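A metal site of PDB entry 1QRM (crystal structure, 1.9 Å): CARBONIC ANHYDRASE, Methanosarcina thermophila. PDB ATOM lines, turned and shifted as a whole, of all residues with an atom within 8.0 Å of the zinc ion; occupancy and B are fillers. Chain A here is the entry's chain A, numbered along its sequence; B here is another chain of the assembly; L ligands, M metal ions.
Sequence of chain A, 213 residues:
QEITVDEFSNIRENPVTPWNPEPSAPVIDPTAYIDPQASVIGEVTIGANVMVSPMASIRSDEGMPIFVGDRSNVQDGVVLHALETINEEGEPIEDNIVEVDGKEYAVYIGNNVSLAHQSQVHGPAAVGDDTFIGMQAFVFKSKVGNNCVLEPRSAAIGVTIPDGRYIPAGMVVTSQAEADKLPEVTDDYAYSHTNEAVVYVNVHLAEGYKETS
Within 4 Å of the zinc ion: His 81, His 122 and His 117 of chain B.
The nearest printed residue that does not touch the zinc ion is Gln 75 of chain B (4.02 Å).
The zinc ion is bound by NE2 of His 122 (2.1 Å), O3 of the ligand (2.2 Å), ND1 of His 81 (2.2 Å), NE2 of His 117 of chain B (2.3 Å) and O4 of the ligand (2.4 Å).
A ring nitrogen (NE2) of His 81 lies within hydrogen-bond range of the guanidinium group (NH1) of Arg 59 (3.4 Å).
The backbone carbonyl oxygen (O) of His 81 is in hydrogen-bond range of the backbone NH (N) of Gly 123, 2.9 Å away.
A ring nitrogen (NE2) of His 81 sits at hydrogen-bond distance from the side-chain carboxylate (OD2) of Asp 61 (2.7 Å).
The backbone NH (N) of His 117 of chain B is in hydrogen-bond range of the side-chain amide oxygen (OE1) of Gln 75 of chain B, at 3.1 Å.
The backbone carbonyl oxygen (O) of His 117 of chain B sits at hydrogen-bond distance from the side-chain amide nitrogen (NE2) of Gln 120, at 3.2 Å.
The side-chain carboxylate of Asp 76 of chain B lies within hydrogen-bond range of a ring nitrogen (ND1) of His 117 of chain B, at 2.6 Å.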
ATOM      1  N   ARG A  59     -28.595  -0.132  15.974  1.00  0.00           N
ATOM      2  CA  ARG A  59     -29.427  -0.905  16.864  1.00  0.00           C
ATOM      3  C   ARG A  59     -28.526  -1.839  17.680  1.00  0.00           C
ATOM      4  O   ARG A  59     -27.957  -2.799  17.172  1.00  0.00           O
ATOM      5  CB  ARG A  59     -30.416  -1.731  16.045  1.00  0.00           C
ATOM      6  CG  ARG A  59     -31.521  -2.497  16.796  1.00  0.00           C
ATOM      7  CD  ARG A  59     -32.642  -2.853  15.842  1.00  0.00           C
ATOM      8  NE  ARG A  59     -32.375  -3.740  14.693  1.00  0.00           N
ATOM      9  CZ  ARG A  59     -32.403  -5.072  14.661  1.00  0.00           C
ATOM     10  NH1 ARG A  59     -32.679  -5.730  15.799  1.00  0.00           N
ATOM     11  NH2 ARG A  59     -32.177  -5.766  13.505  1.00  0.00           N
ATOM     12  N   ASP A  61     -29.255  -4.048  20.329  1.00  0.00           N
ATOM     13  CA  ASP A  61     -30.196  -4.905  21.067  1.00  0.00           C
ATOM     14  C   ASP A  61     -29.831  -6.389  21.119  1.00  0.00           C
ATOM     15  O   ASP A  61     -30.524  -7.185  21.787  1.00  0.00           O
ATOM     16  CB  ASP A  61     -31.603  -4.814  20.428  1.00  0.00           C
ATOM     17  CG  ASP A  61     -31.613  -5.194  18.952  1.00  0.00           C
ATOM     18  OD1 ASP A  61     -32.689  -5.053  18.346  1.00  0.00           O
ATOM     19  OD2 ASP A  61     -30.587  -5.625  18.385  1.00  0.00           O
ATOM     20  N   GLU A  62     -28.762  -6.763  20.436  1.00  0.00           N
ATOM     21  CA  GLU A  62     -28.294  -8.154  20.410  1.00  0.00           C
ATOM     22  C   GLU A  62     -26.871  -8.070  20.937  1.00  0.00           C
ATOM     23  O   GLU A  62     -26.746  -7.942  22.173  1.00  0.00           O
ATOM     24  CB  GLU A  62     -28.487  -8.731  18.989  1.00  0.00           C
ATOM     25  CG  GLU A  62     -28.067 -10.182  18.843  1.00  0.00           C
ATOM     26  CD  GLU A  62     -28.124 -10.733  17.438  1.00  0.00           C
ATOM     27  OE1 GLU A  62     -28.960 -10.212  16.686  1.00  0.00           O
ATOM     28  OE2 GLU A  62     -27.429 -11.732  17.082  1.00  0.00           O
ATOM     29  N   GLY A  63     -25.901  -7.930  20.023  1.00  0.00           N
ATOM     30  CA  GLY A  63     -24.530  -7.611  20.445  1.00  0.00           C
ATOM     31  C   GLY A  63     -24.504  -6.161  20.929  1.00  0.00           C
ATOM     32  O   GLY A  63     -25.126  -5.227  20.362  1.00  0.00           O
ATOM     33  N   VAL A  79     -26.459   0.872   8.293  1.00  0.00           N
ATOM     34  CA  VAL A  79     -26.941   0.047   9.407  1.00  0.00           C
ATOM     35  C   VAL A  79     -25.759  -0.410  10.272  1.00  0.00           C
ATOM     36  O   VAL A  79     -24.722  -0.764   9.699  1.00  0.00           O
ATOM     37  CB  VAL A  79     -27.679  -1.204   8.882  1.00  0.00           C
ATOM     38  CG1 VAL A  79     -28.038  -2.116  10.059  1.00  0.00           C
ATOM     39  CG2 VAL A  79     -28.960  -0.724   8.140  1.00  0.00           C
ATOM     40  N   LEU A  80     -25.901  -0.331  11.576  1.00  0.00           N
ATOM     41  CA  LEU A  80     -24.945  -0.790  12.567  1.00  0.00           C
ATOM     42  C   LEU A  80     -25.732  -1.764  13.467  1.00  0.00           C
ATOM     43  O   LEU A  80     -26.758  -1.381  14.068  1.00  0.00           O
ATOM     44  CB  LEU A  80     -24.367   0.287  13.505  1.00  0.00           C
ATOM     45  CG  LEU A  80     -23.591   1.425  12.833  1.00  0.00           C
ATOM     46  CD1 LEU A  80     -23.020   2.396  13.893  1.00  0.00           C
ATOM     47  CD2 LEU A  80     -22.426   0.883  12.009  1.00  0.00           C
ATOM     48  N   HIS A  81     -25.288  -3.013  13.534  1.00  0.00           N
ATOM     49  CA  HIS A  81     -25.956  -4.043  14.324  1.00  0.00           C
ATOM     50  C   HIS A  81     -24.919  -5.111  14.656  1.00  0.00           C
ATOM     51  O   HIS A  81     -23.815  -4.996  14.090  1.00  0.00           O
ATOM     52  CB  HIS A  81     -27.146  -4.648  13.563  1.00  0.00           C
ATOM     53  CG  HIS A  81     -27.983  -5.486  14.485  1.00  0.00           C
ATOM     54  ND1 HIS A  81     -28.032  -6.855  14.420  1.00  0.00           N
ATOM     55  CD2 HIS A  81     -28.787  -5.119  15.513  1.00  0.00           C
ATOM     56  CE1 HIS A  81     -28.875  -7.332  15.370  1.00  0.00           C
ATOM     57  NE2 HIS A  81     -29.300  -6.280  16.063  1.00  0.00           N
ATOM     58  N   ALA A  82     -25.149  -6.033  15.598  1.00  0.00           N
ATOM     59  CA  ALA A  82     -24.103  -7.025  15.891  1.00  0.00           C
ATOM     60  C   ALA A  82     -24.658  -8.371  16.370  1.00  0.00           C
ATOM     61  O   ALA A  82     -25.773  -8.533  16.860  1.00  0.00           O
ATOM     62  CB  ALA A  82     -23.208  -6.456  17.025  1.00  0.00           C
ATOM     63  N   LEU A  83     -23.823  -9.401  16.205  1.00  0.00           N
ATOM     64  CA  LEU A  83     -24.092 -10.738  16.678  1.00  0.00           C
ATOM     65  C   LEU A  83     -24.096 -10.741  18.198  1.00  0.00           C
ATOM     66  O   LEU A  83     -23.421  -9.938  18.831  1.00  0.00           O
ATOM     67  CB  LEU A  83     -23.038 -11.791  16.229  1.00  0.00           C
ATOM     68  CG  LEU A  83     -22.909 -11.972  14.706  1.00  0.00           C
ATOM     69  CD1 LEU A  83     -21.772 -12.868  14.254  1.00  0.00           C
ATOM     70  CD2 LEU A  83     -24.237 -12.457  14.130  1.00  0.00           C
ATOM     71  N   GLU A  84     -24.889 -11.628  18.784  1.00  0.00           N
ATOM     72  CA  GLU A  84     -24.980 -11.728  20.245  1.00  0.00           C
ATOM     73  C   GLU A  84     -23.645 -11.750  20.954  1.00  0.00           C
ATOM     74  O   GLU A  84     -22.688 -12.434  20.572  1.00  0.00           O
ATOM     75  CB  GLU A  84     -25.842 -12.985  20.563  1.00  0.00           C
ATOM     76  CG  GLU A  84     -26.695 -12.773  21.813  1.00  0.00           C
ATOM     77  CD  GLU A  84     -27.348 -14.069  22.254  1.00  0.00           C
ATOM     78  OE1 GLU A  84     -27.964 -14.731  21.380  1.00  0.00           O
ATOM     79  OE2 GLU A  84     -27.266 -14.444  23.451  1.00  0.00           O
ATOM     80  N   GLN A 120     -22.623  -0.676   5.713  1.00  0.00           N
ATOM     81  CA  GLN A 120     -23.068  -1.400   6.907  1.00  0.00           C
ATOM     82  C   GLN A 120     -21.815  -1.956   7.590  1.00  0.00           C
ATOM     83  O   GLN A 120     -20.916  -2.440   6.917  1.00  0.00           O
ATOM     84  CB  GLN A 120     -23.952  -2.590   6.517  1.00  0.00           C
ATOM     85  CG  GLN A 120     -24.215  -3.626   7.600  1.00  0.00           C
ATOM     86  CD  GLN A 120     -25.255  -4.691   7.272  1.00  0.00           C
ATOM     87  OE1 GLN A 120     -25.399  -5.625   8.076  1.00  0.00           O
ATOM     88  NE2 GLN A 120     -26.013  -4.588   6.188  1.00  0.00           N
ATOM     89  N   VAL A 121     -21.755  -1.853   8.897  1.00  0.00           N
ATOM     90  CA  VAL A 121     -20.683  -2.432   9.708  1.00  0.00           C
ATOM     91  C   VAL A 121     -21.442  -3.310  10.691  1.00  0.00           C
ATOM     92  O   VAL A 121     -22.242  -2.861  11.507  1.00  0.00           O
ATOM     93  CB  VAL A 121     -19.880  -1.347  10.437  1.00  0.00           C
ATOM     94  CG1 VAL A 121     -18.779  -2.003  11.291  1.00  0.00           C
ATOM     95  CG2 VAL A 121     -19.297  -0.367   9.418  1.00  0.00           C
ATOM     96  N   HIS A 122     -21.216  -4.614  10.626  1.00  0.00           N
ATOM     97  CA  HIS A 122     -21.935  -5.541  11.512  1.00  0.00           C
ATOM     98  C   HIS A 122     -20.955  -6.190  12.478  1.00  0.00           C
ATOM     99  O   HIS A 122     -19.958  -6.768  12.023  1.00  0.00           O
ATOM    100  CB  HIS A 122     -22.553  -6.629  10.609  1.00  0.00           C
ATOM    101  CG  HIS A 122     -23.570  -7.367  11.430  1.00  0.00           C
ATOM    102  ND1 HIS A 122     -23.247  -8.308  12.391  1.00  0.00           N
ATOM    103  CD2 HIS A 122     -24.920  -7.263  11.329  1.00  0.00           C
ATOM    104  CE1 HIS A 122     -24.406  -8.738  12.886  1.00  0.00           C
ATOM    105  NE2 HIS A 122     -25.442  -8.124  12.311  1.00  0.00           N
ATOM    106  N   GLY A 123     -21.237  -6.173  13.773  1.00  0.00           N
ATOM    107  CA  GLY A 123     -20.263  -6.748  14.715  1.00  0.00           C
ATOM    108  C   GLY A 123     -20.251  -8.274  14.690  1.00  0.00           C
ATOM    109  O   GLY A 123     -21.222  -8.922  14.291  1.00  0.00           O
ATOM    110  N   PHE A 140     -17.796  -6.929   8.316  1.00  0.00           N
ATOM    111  CA  PHE A 140     -18.422  -7.888   9.198  1.00  0.00           C
ATOM    112  C   PHE A 140     -17.327  -8.832   9.741  1.00  0.00           C
ATOM    113  O   PHE A 140     -16.492  -9.270   8.934  1.00  0.00           O
ATOM    114  CB  PHE A 140     -19.472  -8.698   8.418  1.00  0.00           C
ATOM    115  CG  PHE A 140     -20.105  -9.824   9.191  1.00  0.00           C
ATOM    116  CD1 PHE A 140     -20.477  -9.651  10.520  1.00  0.00           C
ATOM    117  CD2 PHE A 140     -20.351 -11.042   8.593  1.00  0.00           C
ATOM    118  CE1 PHE A 140     -21.071 -10.695  11.221  1.00  0.00           C
ATOM    119  CE2 PHE A 140     -20.942 -12.074   9.288  1.00  0.00           C
ATOM    120  CZ  PHE A 140     -21.308 -11.910  10.620  1.00  0.00           C
ATOM    121  N   GLN B  75     -35.016  -7.648   8.488  1.00  0.00           N
ATOM    122  CA  GLN B  75     -34.113  -6.748   9.152  1.00  0.00           C
ATOM    123  C   GLN B  75     -34.001  -5.356   8.583  1.00  0.00           C
ATOM    124  O   GLN B  75     -34.786  -4.962   7.736  1.00  0.00           O
ATOM    125  CB  GLN B  75     -32.736  -7.411   9.375  1.00  0.00           C
ATOM    126  CG  GLN B  75     -32.840  -8.642  10.271  1.00  0.00           C
ATOM    127  CD  GLN B  75     -31.509  -9.379  10.336  1.00  0.00           C
ATOM    128  OE1 GLN B  75     -30.442  -8.793  10.146  1.00  0.00           O
ATOM    129  NE2 GLN B  75     -31.594 -10.671  10.602  1.00  0.00           N
ATOM    130  N   ASP B  76     -33.136  -4.545   9.230  1.00  0.00           N
ATOM    131  CA  ASP B  76     -33.121  -3.121   8.937  1.00  0.00           C
ATOM    132  C   ASP B  76     -32.878  -2.853   7.454  1.00  0.00           C
ATOM    133  O   ASP B  76     -31.913  -3.356   6.890  1.00  0.00           O
ATOM    134  CB  ASP B  76     -32.005  -2.402   9.725  1.00  0.00           C
ATOM    135  CG  ASP B  76     -31.942  -2.825  11.188  1.00  0.00           C
ATOM    136  OD1 ASP B  76     -31.604  -3.991  11.452  1.00  0.00           O
ATOM    137  OD2 ASP B  76     -32.231  -2.046  12.146  1.00  0.00           O
ATOM    138  N   ALA B 116     -31.580 -10.711   6.304  1.00  0.00           N
ATOM    139  CA  ALA B 116     -30.615  -9.901   7.022  1.00  0.00           C
ATOM    140  C   ALA B 116     -30.512  -8.475   6.494  1.00  0.00           C
ATOM    141  O   ALA B 116     -30.983  -8.096   5.431  1.00  0.00           O
ATOM    142  CB  ALA B 116     -29.307 -10.641   7.115  1.00  0.00           C
ATOM    143  N   HIS B 117     -29.945  -7.593   7.315  1.00  0.00           N
ATOM    144  CA  HIS B 117     -29.904  -6.164   7.059  1.00  0.00           C
ATOM    145  C   HIS B 117     -29.546  -5.784   5.633  1.00  0.00           C
ATOM    146  O   HIS B 117     -28.524  -6.199   5.048  1.00  0.00           O
ATOM    147  CB  HIS B 117     -28.889  -5.454   7.986  1.00  0.00           C
ATOM    148  CG  HIS B 117     -28.883  -5.907   9.396  1.00  0.00           C
ATOM    149  ND1 HIS B 117     -29.815  -5.441  10.334  1.00  0.00           N
ATOM    150  CD2 HIS B 117     -28.026  -6.792  10.016  1.00  0.00           C
ATOM    151  CE1 HIS B 117     -29.529  -6.028  11.491  1.00  0.00           C
ATOM    152  NE2 HIS B 117     -28.487  -6.791  11.288  1.00  0.00           N
ATOM    153  N   PHE B 132     -31.172 -18.516   5.401  1.00  0.00           N
ATOM    154  CA  PHE B 132     -30.609 -17.239   5.815  1.00  0.00           C
ATOM    155  C   PHE B 132     -30.302 -16.448   4.526  1.00  0.00           C
ATOM    156  O   PHE B 132     -29.501 -16.914   3.695  1.00  0.00           O
ATOM    157  CB  PHE B 132     -29.338 -17.426   6.642  1.00  0.00           C
ATOM    158  CG  PHE B 132     -28.600 -16.190   7.095  1.00  0.00           C
ATOM    159  CD1 PHE B 132     -29.001 -15.500   8.221  1.00  0.00           C
ATOM    160  CD2 PHE B 132     -27.505 -15.745   6.380  1.00  0.00           C
ATOM    161  CE1 PHE B 132     -28.305 -14.361   8.641  1.00  0.00           C
ATOM    162  CE2 PHE B 132     -26.799 -14.622   6.806  1.00  0.00           C
ATOM    163  CZ  PHE B 132     -27.213 -13.928   7.932  1.00  0.00           C
ATOM    164  N   MET B 135     -26.615 -10.328   4.606  1.00  0.00           N
ATOM    165  CA  MET B 135     -26.582  -8.886   4.595  1.00  0.00           C
ATOM    166  C   MET B 135     -26.270  -8.377   3.194  1.00  0.00           C
ATOM    167  O   MET B 135     -25.382  -8.843   2.458  1.00  0.00           O
ATOM    168  CB  MET B 135     -25.541  -8.331   5.592  1.00  0.00           C
ATOM    169  CG  MET B 135     -25.674  -8.671   7.066  1.00  0.00           C
ATOM    170  SD  MET B 135     -24.995 -10.307   7.456  1.00  0.00           S
ATOM    171  CE  MET B 135     -25.196 -10.394   9.228  1.00  0.00           C
ATOM    172  N   VAL B 198     -30.101 -16.850  14.557  1.00  0.00           N
ATOM    173  CA  VAL B 198     -30.735 -15.595  14.186  1.00  0.00           C
ATOM    174  C   VAL B 198     -32.246 -15.639  14.439  1.00  0.00           C
ATOM    175  O   VAL B 198     -32.881 -14.698  14.935  1.00  0.00           O
ATOM    176  CB  VAL B 198     -30.423 -15.214  12.734  1.00  0.00           C
ATOM    177  CG1 VAL B 198     -31.051 -13.873  12.354  1.00  0.00           C
ATOM    178  CG2 VAL B 198     -28.910 -15.144  12.513  1.00  0.00           C
ATOM    179  N   VAL B 201     -32.889 -15.517  18.215  1.00  0.00           N
ATOM    180  CA  VAL B 201     -32.730 -14.134  18.637  1.00  0.00           C
ATOM    181  C   VAL B 201     -33.898 -13.249  18.251  1.00  0.00           C
ATOM    182  O   VAL B 201     -34.466 -12.528  19.068  1.00  0.00           O
ATOM    183  CB  VAL B 201     -31.414 -13.561  18.051  1.00  0.00           C
ATOM    184  CG1 VAL B 201     -31.386 -12.034  18.146  1.00  0.00           C
ATOM    185  CG2 VAL B 201     -30.226 -14.158  18.756  1.00  0.00           C
ATOM    186  N   ASN B 202     -34.278 -13.199  16.980  1.00  0.00           N
ATOM    187  CA  ASN B 202     -35.342 -12.364  16.484  1.00  0.00           C
ATOM    188  C   ASN B 202     -36.723 -12.705  17.015  1.00  0.00           C
ATOM    189  O   ASN B 202     -37.577 -11.842  17.187  1.00  0.00           O
ATOM    190  CB  ASN B 202     -35.358 -12.308  14.943  1.00  0.00           C
ATOM    191  CG  ASN B 202     -34.247 -11.372  14.413  1.00  0.00           C
ATOM    192  OD1 ASN B 202     -34.598 -10.201  14.183  1.00  0.00           O
ATOM    193  ND2 ASN B 202     -33.033 -11.851  14.274  1.00  0.00           N
ATOM    194  N   LEU B 205     -36.501 -10.992  20.218  1.00  0.00           N
ATOM    195  CA  LEU B 205     -36.554  -9.545  20.063  1.00  0.00           C
ATOM    196  C   LEU B 205     -37.985  -9.105  19.814  1.00  0.00           C
ATOM    197  O   LEU B 205     -38.456  -8.102  20.348  1.00  0.00           O
ATOM    198  CB  LEU B 205     -35.653  -8.961  18.946  1.00  0.00           C
ATOM    199  CG  LEU B 205     -34.170  -8.917  19.265  1.00  0.00           C
ATOM    200  CD1 LEU B 205     -33.321  -8.672  18.007  1.00  0.00           C
ATOM    201  CD2 LEU B 205     -33.869  -7.833  20.302  1.00  0.00           C
HETATM  202  S1  LIG L   1     -27.869 -11.014  13.355  1.00  0.00           S
HETATM  203  O1  LIG L   1     -28.750 -11.739  14.288  1.00  0.00           O
HETATM  204  O2  LIG L   1     -27.118 -11.832  12.344  1.00  0.00           O
HETATM  205  O3  LIG L   1     -28.687  -9.988  12.556  1.00  0.00           O
HETATM  206  O4  LIG L   1     -26.912 -10.124  14.137  1.00  0.00           O
HETATM  207 ZN    ZN M   1     -27.491  -8.202  12.805  1.00  0.00          ZN
